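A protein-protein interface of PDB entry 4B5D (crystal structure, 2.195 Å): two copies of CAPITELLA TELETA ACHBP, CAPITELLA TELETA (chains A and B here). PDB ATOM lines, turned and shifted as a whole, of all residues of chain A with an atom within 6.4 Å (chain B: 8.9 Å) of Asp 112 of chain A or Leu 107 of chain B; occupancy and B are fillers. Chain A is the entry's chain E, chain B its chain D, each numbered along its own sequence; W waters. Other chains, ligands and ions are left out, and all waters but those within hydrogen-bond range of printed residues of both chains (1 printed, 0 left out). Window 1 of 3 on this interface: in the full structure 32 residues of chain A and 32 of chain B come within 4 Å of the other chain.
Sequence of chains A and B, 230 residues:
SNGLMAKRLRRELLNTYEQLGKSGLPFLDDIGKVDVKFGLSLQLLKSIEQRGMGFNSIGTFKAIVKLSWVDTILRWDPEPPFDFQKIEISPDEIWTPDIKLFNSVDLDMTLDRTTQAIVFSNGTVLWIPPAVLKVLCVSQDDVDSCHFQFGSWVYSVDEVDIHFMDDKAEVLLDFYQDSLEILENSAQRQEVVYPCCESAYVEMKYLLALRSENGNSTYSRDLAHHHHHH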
ATOM      1  N   LYS A  62     -23.984  36.089   8.610  1.00  0.00           N
ATOM      2  CA  LYS A  62     -22.995  35.138   9.088  1.00  0.00           C
ATOM      3  C   LYS A  62     -21.880  35.029   8.039  1.00  0.00           C
ATOM      4  O   LYS A  62     -22.131  34.863   6.822  1.00  0.00           O
ATOM      5  CB  LYS A  62     -23.650  33.773   9.333  1.00  0.00           C
ATOM      6  CG  LYS A  62     -22.663  32.632   9.525  1.00  0.00           C
ATOM      7  CD  LYS A  62     -21.984  32.702  10.891  1.00  0.00           C
ATOM      8  CE  LYS A  62     -20.881  31.652  11.000  1.00  0.00           C
ATOM      9  NZ  LYS A  62     -21.350  30.292  10.566  1.00  0.00           N
ATOM     10  N   ALA A  63     -20.644  35.130   8.507  1.00  0.00           N
ATOM     11  CA  ALA A  63     -19.502  35.144   7.596  1.00  0.00           C
ATOM     12  C   ALA A  63     -18.272  34.516   8.214  1.00  0.00           C
ATOM     13  O   ALA A  63     -18.265  34.146   9.386  1.00  0.00           O
ATOM     14  CB  ALA A  63     -19.188  36.566   7.165  1.00  0.00           C
ATOM     15  N   PRO A  91      -5.995  32.518  19.865  1.00  0.00           N
ATOM     16  CA  PRO A  91      -5.848  33.962  19.607  1.00  0.00           C
ATOM     17  C   PRO A  91      -5.849  34.830  20.871  1.00  0.00           C
ATOM     18  O   PRO A  91      -5.396  35.977  20.827  1.00  0.00           O
ATOM     19  CB  PRO A  91      -7.063  34.305  18.740  1.00  0.00           C
ATOM     20  CG  PRO A  91      -7.987  33.144  18.841  1.00  0.00           C
ATOM     21  CD  PRO A  91      -7.184  31.938  19.219  1.00  0.00           C
ATOM     22  N   THR A 110     -19.076  40.200  16.222  1.00  0.00           N
ATOM     23  CA  THR A 110     -18.550  39.203  17.132  1.00  0.00           C
ATOM     24  C   THR A 110     -17.771  38.163  16.337  1.00  0.00           C
ATOM     25  O   THR A 110     -18.274  37.582  15.356  1.00  0.00           O
ATOM     26  CB  THR A 110     -19.651  38.529  17.962  1.00  0.00           C
ATOM     27  OG1 THR A 110     -20.607  37.937  17.081  1.00  0.00           O
ATOM     28  CG2 THR A 110     -20.363  39.541  18.862  1.00  0.00           C
ATOM     29  N   LEU A 111     -16.526  37.962  16.745  1.00  0.00           N
ATOM     30  CA  LEU A 111     -15.691  36.922  16.160  1.00  0.00           C
ATOM     31  C   LEU A 111     -15.657  35.756  17.129  1.00  0.00           C
ATOM     32  O   LEU A 111     -15.631  35.960  18.344  1.00  0.00           O
ATOM     33  CB  LEU A 111     -14.271  37.438  15.939  1.00  0.00           C
ATOM     34  CG  LEU A 111     -14.030  38.624  15.009  1.00  0.00           C
ATOM     35  CD1 LEU A 111     -12.557  38.984  15.024  1.00  0.00           C
ATOM     36  CD2 LEU A 111     -14.496  38.338  13.580  1.00  0.00           C
ATOM     37  N   ASP A 112     -15.651  34.537  16.602  1.00  0.00           N
ATOM     38  CA  ASP A 112     -15.539  33.360  17.452  1.00  0.00           C
ATOM     39  C   ASP A 112     -14.086  33.207  17.885  1.00  0.00           C
ATOM     40  O   ASP A 112     -13.262  32.628  17.169  1.00  0.00           O
ATOM     41  CB  ASP A 112     -16.027  32.111  16.715  1.00  0.00           C
ATOM     42  CG  ASP A 112     -16.128  30.887  17.615  1.00  0.00           C
ATOM     43  OD1 ASP A 112     -15.586  30.916  18.740  1.00  0.00           O
ATOM     44  OD2 ASP A 112     -16.742  29.879  17.179  1.00  0.00           O
ATOM     45  N   ARG A 113     -13.775  33.715  19.073  1.00  0.00           N
ATOM     46  CA  ARG A 113     -12.391  33.689  19.547  1.00  0.00           C
ATOM     47  C   ARG A 113     -11.953  32.343  20.121  1.00  0.00           C
ATOM     48  O   ARG A 113     -10.795  32.180  20.477  1.00  0.00           O
ATOM     49  CB  ARG A 113     -12.118  34.843  20.524  1.00  0.00           C
ATOM     50  CG  ARG A 113     -12.289  36.210  19.879  1.00  0.00           C
ATOM     51  CD  ARG A 113     -11.836  37.369  20.781  1.00  0.00           C
ATOM     52  NE  ARG A 113     -10.392  37.558  20.714  1.00  0.00           N
ATOM     53  CZ  ARG A 113      -9.783  38.283  19.779  1.00  0.00           C
ATOM     54  NH1 ARG A 113     -10.499  38.900  18.842  1.00  0.00           N
ATOM     55  NH2 ARG A 113      -8.458  38.400  19.785  1.00  0.00           N
ATOM     56  N   THR A 114     -12.858  31.368  20.185  1.00  0.00           N
ATOM     57  CA  THR A 114     -12.435  30.006  20.537  1.00  0.00           C
ATOM     58  C   THR A 114     -11.684  29.354  19.376  1.00  0.00           C
ATOM     59  O   THR A 114     -11.000  28.350  19.555  1.00  0.00           O
ATOM     60  CB  THR A 114     -13.622  29.065  20.945  1.00  0.00           C
ATOM     61  OG1 THR A 114     -14.427  28.762  19.801  1.00  0.00           O
ATOM     62  CG2 THR A 114     -14.497  29.704  22.026  1.00  0.00           C
ATOM     63  N   THR A 115     -11.841  29.922  18.183  1.00  0.00           N
ATOM     64  CA  THR A 115     -11.232  29.400  16.968  1.00  0.00           C
ATOM     65  C   THR A 115      -9.721  29.576  17.008  1.00  0.00           C
ATOM     66  O   THR A 115      -9.249  30.698  17.178  1.00  0.00           O
ATOM     67  CB  THR A 115     -11.711  30.187  15.744  1.00  0.00           C
ATOM     68  OG1 THR A 115     -13.143  30.243  15.724  1.00  0.00           O
ATOM     69  CG2 THR A 115     -11.215  29.536  14.487  1.00  0.00           C
ATOM     70  N   GLN A 116      -8.964  28.493  16.822  1.00  0.00           N
ATOM     71  CA  GLN A 116      -7.507  28.585  16.871  1.00  0.00           C
ATOM     72  C   GLN A 116      -6.924  29.272  15.648  1.00  0.00           C
ATOM     73  O   GLN A 116      -7.502  29.226  14.564  1.00  0.00           O
ATOM     74  CB  GLN A 116      -6.882  27.208  17.007  1.00  0.00           C
ATOM     75  CG  GLN A 116      -7.421  26.402  18.152  1.00  0.00           C
ATOM     76  CD  GLN A 116      -6.841  25.007  18.168  1.00  0.00           C
ATOM     77  OE1 GLN A 116      -5.867  24.742  18.878  1.00  0.00           O
ATOM     78  NE2 GLN A 116      -7.426  24.107  17.368  1.00  0.00           N
ATOM     79  N   TRP A 127      -5.423  33.322  10.836  1.00  0.00           N
ATOM     80  CA  TRP A 127      -6.546  33.196  11.779  1.00  0.00           C
ATOM     81  C   TRP A 127      -7.817  33.445  11.009  1.00  0.00           C
ATOM     82  O   TRP A 127      -7.989  34.502  10.388  1.00  0.00           O
ATOM     83  CB  TRP A 127      -6.447  34.215  12.910  1.00  0.00           C
ATOM     84  CG  TRP A 127      -7.518  34.070  13.971  1.00  0.00           C
ATOM     85  CD1 TRP A 127      -8.073  32.901  14.435  1.00  0.00           C
ATOM     86  CD2 TRP A 127      -8.163  35.134  14.698  1.00  0.00           C
ATOM     87  NE1 TRP A 127      -9.014  33.180  15.402  1.00  0.00           N
ATOM     88  CE2 TRP A 127      -9.091  34.536  15.581  1.00  0.00           C
ATOM     89  CE3 TRP A 127      -8.042  36.529  14.691  1.00  0.00           C
ATOM     90  CZ2 TRP A 127      -9.897  35.287  16.437  1.00  0.00           C
ATOM     91  CZ3 TRP A 127      -8.837  37.276  15.548  1.00  0.00           C
ATOM     92  CH2 TRP A 127      -9.747  36.653  16.416  1.00  0.00           C
ATOM     93  N   PRO A 129     -11.554  33.295  11.877  1.00  0.00           N
ATOM     94  CA  PRO A 129     -12.756  33.057  12.698  1.00  0.00           C
ATOM     95  C   PRO A 129     -14.088  33.251  11.969  1.00  0.00           C
ATOM     96  O   PRO A 129     -14.231  34.153  11.138  1.00  0.00           O
ATOM     97  CB  PRO A 129     -12.632  34.098  13.818  1.00  0.00           C
ATOM     98  CG  PRO A 129     -11.895  35.263  13.152  1.00  0.00           C
ATOM     99  CD  PRO A 129     -10.851  34.538  12.265  1.00  0.00           C
ATOM    100  N   PRO A 130     -15.065  32.390  12.277  1.00  0.00           N
ATOM    101  CA  PRO A 130     -16.448  32.721  11.915  1.00  0.00           C
ATOM    102  C   PRO A 130     -16.899  34.013  12.611  1.00  0.00           C
ATOM    103  O   PRO A 130     -16.401  34.363  13.679  1.00  0.00           O
ATOM    104  CB  PRO A 130     -17.242  31.518  12.441  1.00  0.00           C
ATOM    105  CG  PRO A 130     -16.253  30.361  12.383  1.00  0.00           C
ATOM    106  CD  PRO A 130     -14.912  30.995  12.736  1.00  0.00           C
ATOM    107  N   ALA A 131     -17.850  34.710  12.009  1.00  0.00           N
ATOM    108  CA  ALA A 131     -18.271  36.000  12.521  1.00  0.00           C
ATOM    109  C   ALA A 131     -19.744  36.257  12.247  1.00  0.00           C
ATOM    110  O   ALA A 131     -20.304  35.762  11.264  1.00  0.00           O
ATOM    111  CB  ALA A 131     -17.407  37.128  11.926  1.00  0.00           C
ATOM    112  N   VAL A 132     -20.365  37.026  13.138  1.00  0.00           N
ATOM    113  CA  VAL A 132     -21.703  37.557  12.926  1.00  0.00           C
ATOM    114  C   VAL A 132     -21.635  39.089  12.763  1.00  0.00           C
ATOM    115  O   VAL A 132     -21.057  39.777  13.599  1.00  0.00           O
ATOM    116  CB  VAL A 132     -22.647  37.192  14.107  1.00  0.00           C
ATOM    117  CG1 VAL A 132     -23.950  38.033  14.042  1.00  0.00           C
ATOM    118  CG2 VAL A 132     -22.948  35.692  14.115  1.00  0.00           C
ATOM    119  N   ASP B  98     -11.615  20.573  17.725  1.00  0.00           N
ATOM    120  CA  ASP B  98     -12.215  21.888  17.459  1.00  0.00           C
ATOM    121  C   ASP B  98     -13.361  21.744  16.455  1.00  0.00           C
ATOM    122  O   ASP B  98     -13.410  22.439  15.431  1.00  0.00           O
ATOM    123  CB  ASP B  98     -11.164  22.871  16.931  1.00  0.00           C
ATOM    124  CG  ASP B  98     -10.515  22.383  15.641  1.00  0.00           C
ATOM    125  OD1 ASP B  98     -10.552  21.150  15.395  1.00  0.00           O
ATOM    126  OD2 ASP B  98      -9.996  23.220  14.864  1.00  0.00           O
ATOM    127  N   ILE B  99     -14.285  20.834  16.747  1.00  0.00           N
ATOM    128  CA  ILE B  99     -15.354  20.524  15.810  1.00  0.00           C
ATOM    129  C   ILE B  99     -16.413  21.621  15.814  1.00  0.00           C
ATOM    130  O   ILE B  99     -16.977  21.935  16.859  1.00  0.00           O
ATOM    131  CB  ILE B  99     -15.996  19.167  16.123  1.00  0.00           C
ATOM    132  CG1 ILE B  99     -15.030  18.033  15.751  1.00  0.00           C
ATOM    133  CG2 ILE B  99     -17.284  19.019  15.355  1.00  0.00           C
ATOM    134  CD1 ILE B  99     -15.442  16.677  16.269  1.00  0.00           C
ATOM    135  N   LYS B 100     -16.655  22.218  14.647  1.00  0.00           N
ATOM    136  CA  LYS B 100     -17.652  23.284  14.528  1.00  0.00           C
ATOM    137  C   LYS B 100     -18.822  22.918  13.612  1.00  0.00           C
ATOM    138  O   LYS B 100     -18.696  22.075  12.701  1.00  0.00           O
ATOM    139  CB  LYS B 100     -17.012  24.588  14.037  1.00  0.00           C
ATOM    140  CG  LYS B 100     -16.091  25.276  15.038  1.00  0.00           C
ATOM    141  CD  LYS B 100     -15.442  26.528  14.422  1.00  0.00           C
ATOM    142  CE  LYS B 100     -15.212  27.630  15.466  1.00  0.00           C
ATOM    143  NZ  LYS B 100     -14.557  27.169  16.740  1.00  0.00           N
ATOM    144  N   LEU B 101     -19.960  23.556  13.876  1.00  0.00           N
ATOM    145  CA  LEU B 101     -21.098  23.514  12.976  1.00  0.00           C
ATOM    146  C   LEU B 101     -20.863  24.621  11.966  1.00  0.00           C
ATOM    147  O   LEU B 101     -21.015  25.805  12.289  1.00  0.00           O
ATOM    148  CB  LEU B 101     -22.389  23.754  13.756  1.00  0.00           C
ATOM    149  CG  LEU B 101     -23.705  23.848  12.989  1.00  0.00           C
ATOM    150  CD1 LEU B 101     -23.985  22.532  12.263  1.00  0.00           C
ATOM    151  CD2 LEU B 101     -24.852  24.187  13.967  1.00  0.00           C
ATOM    152  N   PHE B 102     -20.468  24.239  10.756  1.00  0.00           N
ATOM    153  CA  PHE B 102     -19.958  25.195   9.775  1.00  0.00           C
ATOM    154  C   PHE B 102     -21.071  26.099   9.278  1.00  0.00           C
ATOM    155  O   PHE B 102     -20.898  27.311   9.164  1.00  0.00           O
ATOM    156  CB  PHE B 102     -19.327  24.474   8.578  1.00  0.00           C
ATOM    157  CG  PHE B 102     -18.010  23.803   8.878  1.00  0.00           C
ATOM    158  CD1 PHE B 102     -17.541  23.686  10.176  1.00  0.00           C
ATOM    159  CD2 PHE B 102     -17.240  23.289   7.850  1.00  0.00           C
ATOM    160  CE1 PHE B 102     -16.332  23.071  10.444  1.00  0.00           C
ATOM    161  CE2 PHE B 102     -16.027  22.667   8.112  1.00  0.00           C
ATOM    162  CZ  PHE B 102     -15.574  22.561   9.413  1.00  0.00           C
ATOM    163  N   ASN B 103     -22.224  25.501   8.995  1.00  0.00           N
ATOM    164  CA  ASN B 103     -23.359  26.246   8.467  1.00  0.00           C
ATOM    165  C   ASN B 103     -24.233  26.839   9.564  1.00  0.00           C
ATOM    166  O   ASN B 103     -25.416  27.118   9.348  1.00  0.00           O
ATOM    167  CB  ASN B 103     -24.192  25.369   7.531  1.00  0.00           C
ATOM    168  CG  ASN B 103     -24.846  24.213   8.247  1.00  0.00           C
ATOM    169  OD1 ASN B 103     -24.220  23.523   9.059  1.00  0.00           O
ATOM    170  ND2 ASN B 103     -26.121  24.002   7.964  1.00  0.00           N
ATOM    171  N   SER B 104     -23.644  27.033  10.741  1.00  0.00           N
ATOM    172  CA  SER B 104     -24.329  27.714  11.833  1.00  0.00           C
ATOM    173  C   SER B 104     -24.771  29.108  11.418  1.00  0.00           C
ATOM    174  O   SER B 104     -24.010  29.865  10.803  1.00  0.00           O
ATOM    175  CB  SER B 104     -23.434  27.821  13.062  1.00  0.00           C
ATOM    176  OG  SER B 104     -24.064  28.610  14.057  1.00  0.00           O
ATOM    177  N   VAL B 105     -26.015  29.426  11.751  1.00  0.00           N
ATOM    178  CA  VAL B 105     -26.582  30.753  11.531  1.00  0.00           C
ATOM    179  C   VAL B 105     -25.994  31.763  12.547  1.00  0.00           C
ATOM    180  O   VAL B 105     -25.963  32.973  12.300  1.00  0.00           O
ATOM    181  CB  VAL B 105     -28.128  30.659  11.600  1.00  0.00           C
ATOM    182  CG1 VAL B 105     -28.738  31.907  12.126  1.00  0.00           C
ATOM    183  CG2 VAL B 105     -28.711  30.297  10.231  1.00  0.00           C
ATOM    184  N   ASP B 106     -25.514  31.239  13.677  1.00  0.00           N
ATOM    185  CA  ASP B 106     -24.743  32.010  14.656  1.00  0.00           C
ATOM    186  C   ASP B 106     -23.264  31.706  14.480  1.00  0.00           C
ATOM    187  O   ASP B 106     -22.872  31.144  13.451  1.00  0.00           O
ATOM    188  CB  ASP B 106     -25.146  31.619  16.072  1.00  0.00           C
ATOM    189  CG  ASP B 106     -26.560  32.024  16.409  1.00  0.00           C
ATOM    190  OD1 ASP B 106     -27.061  32.992  15.790  1.00  0.00           O
ATOM    191  OD2 ASP B 106     -27.162  31.366  17.288  1.00  0.00           O
ATOM    192  N   LEU B 107     -22.448  32.069  15.475  1.00  0.00           N
ATOM    193  CA  LEU B 107     -20.999  31.860  15.390  1.00  0.00           C
ATOM    194  C   LEU B 107     -20.679  30.388  15.236  1.00  0.00           C
ATOM    195  O   LEU B 107     -19.826  30.005  14.432  1.00  0.00           O
ATOM    196  CB  LEU B 107     -20.277  32.393  16.629  1.00  0.00           C
ATOM    197  CG  LEU B 107     -19.969  33.881  16.708  1.00  0.00           C
ATOM    198  CD1 LEU B 107     -19.202  34.164  17.992  1.00  0.00           C
ATOM    199  CD2 LEU B 107     -19.173  34.316  15.475  1.00  0.00           C
ATOM    200  N   ASP B 108     -21.374  29.572  16.027  1.00  0.00           N
ATOM    201  CA  ASP B 108     -21.191  28.130  16.018  1.00  0.00           C
ATOM    202  C   ASP B 108     -22.375  27.537  16.779  1.00  0.00           C
ATOM    203  O   ASP B 108     -23.191  28.271  17.343  1.00  0.00           O
ATOM    204  CB  ASP B 108     -19.863  27.759  16.699  1.00  0.00           C
ATOM    205  CG  ASP B 108     -19.458  26.279  16.490  1.00  0.00           C
ATOM    206  OD1 ASP B 108     -20.104  25.562  15.689  1.00  0.00           O
ATOM    207  OD2 ASP B 108     -18.473  25.841  17.131  1.00  0.00           O
ATOM    208  N   MET B 109     -22.478  26.214  16.780  1.00  0.00           N
ATOM    209  CA  MET B 109     -23.374  25.533  17.696  1.00  0.00           C
ATOM    210  C   MET B 109     -22.909  25.840  19.123  1.00  0.00           C
ATOM    211  O   MET B 109     -21.759  26.194  19.352  1.00  0.00           O
ATOM    212  CB  MET B 109     -23.355  24.015  17.438  1.00  0.00           C
ATOM    213  CG  MET B 109     -22.035  23.320  17.781  1.00  0.00           C
ATOM    214  SD  MET B 109     -21.960  21.534  17.386  1.00  0.00           S
ATOM    215  CE  MET B 109     -23.623  21.059  17.834  1.00  0.00           C
ATOM    216  N   THR B 110     -23.806  25.727  20.086  1.00  0.00           N
ATOM    217  CA  THR B 110     -23.379  25.830  21.469  1.00  0.00           C
ATOM    218  C   THR B 110     -23.419  24.436  22.100  1.00  0.00           C
ATOM    219  O   THR B 110     -24.429  23.748  22.038  1.00  0.00           O
ATOM    220  CB  THR B 110     -24.228  26.873  22.264  1.00  0.00           C
ATOM    221  OG1 THR B 110     -25.614  26.694  21.962  1.00  0.00           O
ATOM    222  CG2 THR B 110     -23.847  28.308  21.874  1.00  0.00           C
ATOM    223  N   LYS B 134     -28.529  25.897  15.184  1.00  0.00           N
ATOM    224  CA  LYS B 134     -29.336  26.862  14.459  1.00  0.00           C
ATOM    225  C   LYS B 134     -28.830  26.945  13.024  1.00  0.00           C
ATOM    226  O   LYS B 134     -27.716  27.407  12.772  1.00  0.00           O
ATOM    227  CB  LYS B 134     -29.275  28.223  15.144  1.00  0.00           C
ATOM    228  CG  LYS B 134     -30.389  29.172  14.746  1.00  0.00           C
ATOM    229  CD  LYS B 134     -30.480  30.355  15.712  1.00  0.00           C
ATOM    230  CE  LYS B 134     -30.594  29.871  17.154  1.00  0.00           C
ATOM    231  NZ  LYS B 134     -31.501  30.727  17.975  1.00  0.00           N
ATOM    232  N   TRP B 153     -12.083  22.654  12.510  1.00  0.00           N
ATOM    233  CA  TRP B 153     -11.811  23.889  11.791  1.00  0.00           C
ATOM    234  C   TRP B 153     -10.404  23.934  11.197  1.00  0.00           C
ATOM    235  O   TRP B 153     -10.238  24.218  10.011  1.00  0.00           O
ATOM    236  CB  TRP B 153     -12.054  25.107  12.687  1.00  0.00           C
ATOM    237  CG  TRP B 153     -12.200  26.385  11.905  1.00  0.00           C
ATOM    238  CD1 TRP B 153     -11.337  27.437  11.884  1.00  0.00           C
ATOM    239  CD2 TRP B 153     -13.271  26.723  11.018  1.00  0.00           C
ATOM    240  NE1 TRP B 153     -11.806  28.416  11.043  1.00  0.00           N
ATOM    241  CE2 TRP B 153     -12.996  28.005  10.502  1.00  0.00           C
ATOM    242  CE3 TRP B 153     -14.443  26.068  10.617  1.00  0.00           C
ATOM    243  CZ2 TRP B 153     -13.851  28.654   9.596  1.00  0.00           C
ATOM    244  CZ3 TRP B 153     -15.297  26.710   9.721  1.00  0.00           C
ATOM    245  CH2 TRP B 153     -14.995  27.990   9.219  1.00  0.00           C
HETATM  246  O   HOH W   1      -9.831  25.961  16.228  1.00  0.00           O
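The side-chain amino group of Lys 100 of chain B lies within salt-bridge range of the side-chain carboxylate of Asp 112 of chain A, 3.5 Å away.
The side-chain hydroxyl (OG1) of Thr 114 of chain A lies within hydrogen-bond range of the side-chain amino group (NZ) of Lys 100 of chain B (3.5 Å).
O of Phe 102 of chain B sits at hydrogen-bond distance from NZ of Lys 62 of chain A, at 3.3 Å.
NZ of Lys 62 of chain A sits at hydrogen-bond distance from O of Ser 104 of chain B (2.7 Å).
NZ of Lys 62 of chain A sits close to O of Asp 106 of chain B, 3.4 Å away.
The backbone carbonyl oxygen (O) of Asp 108 of chain B sits close to the side-chain hydroxyl (OG) of Ser 104 of chain B, 3.4 Å away.
The backbone carbonyl oxygen (O) of Ala 63 of chain A sits at hydrogen-bond distance from the backbone NH (N) of Ala 131 of chain A (2.7 Å).
The backbone carbonyl oxygen (O) of Thr 110 of chain A lies within hydrogen-bond range of the backbone NH (N) of Val 132 of chain A, 3.1 Å away.
The side-chain carboxylate (OD1) of Asp 112 of chain A lies within hydrogen-bond range of the side-chain hydroxyl (OG1) of Thr 114 of chain A, 2.7 Å away.
O of Asp 112 of chain A lies within hydrogen-bond range of OG1 of Thr 115 of chain A (2.8 Å).
The backbone NH (N) of Asp 112 of chain A is in hydrogen-bond range of the backbone carbonyl oxygen (O) of Pro 130 of chain A (3.0 Å).
Among the printed residues, merely in contact across the chains: Lys 62 of chain A with Val 105 of chain B (3.8 Å), Lys 62 of chain A with Leu 107 of chain B (3.95 Å), Thr 110 of chain A with Leu 107 of chain B (3.4 Å), Leu 111 of chain A with Leu 107 of chain B (3.98 Å), Asp 112 of chain A with Leu 107 of chain B (3.7 Å), Asp 112 of chain A with Asp 108 of chain B (3.8 Å), Thr 115 of chain A with Lys 100 of chain B (3.3 Å), Thr 115 of chain A with Trp 153 of chain B (3.3 Å), Gln 116 of chain A with Asp 98 of chain B (3.7 Å), Pro 130 of chain A with Leu 107 of chain B (3.3 Å), Ala 131 of chain A with Leu 107 of chain B (3.5 Å) and Val 132 of chain A with Leu 107 of chain B (3.8 Å).
Printed residues of chain B within 4 Å of Thr 110 of chain A: Leu 107 (3.4 Å).
Of chain B, only Lys 100, Leu 107 and Asp 108 come within 4 Å of Asp 112 of chain A.
Of chain B, only Leu 107 comes within 4 Å of Pro 130 of chain A.
Of the printed residues of chain A, Ser 104 of chain B touches Lys 62 (2.7 Å).
Of the printed residues of chain A, Leu 107 of chain B touches Lys 62 (3.95 Å), Thr 110 (3.4 Å), Leu 111 (3.98 Å), Asp 112 (3.7 Å), Pro 130 (3.3 Å), Ala 131 (3.5 Å) and Val 132 (3.8 Å).
Printed residues of chain A within 4 Å of Asp 108 of chain B: Asp 112.
Lys 134 of chain B touches none of the printed residues of chain A.
Of the 15 printed residues of chain B, 9 touch a printed residue of chain A.
Hydrophobic or aromatic side chains of chain B that line the printed part of chain A: Leu 107 and Trp 153.
Of the 15 printed residues of chain A, 10 touch a printed residue of chain B.
Printed residues of chain A that touch a printed residue of chain B: Lys 62, Thr 110, Leu 111, Asp 112, Thr 114, Thr 115, Gln 116, Pro 130, Ala 131 and Val 132.
Among the printed residues, 17 pairs touch across the chains.
Among the printed residues, Asp or Glu carboxylates within 4 Å of a Lys or Arg side-chain nitrogen of the other chain: Asp 112 of chain A with Lys 100 of chain B (3.5 Å).
1 position is printed for both chains.
Water W1 bridges the backbone NH of Gln 116 of chain A and the side-chain carboxylate of Asp 98 of chain B.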
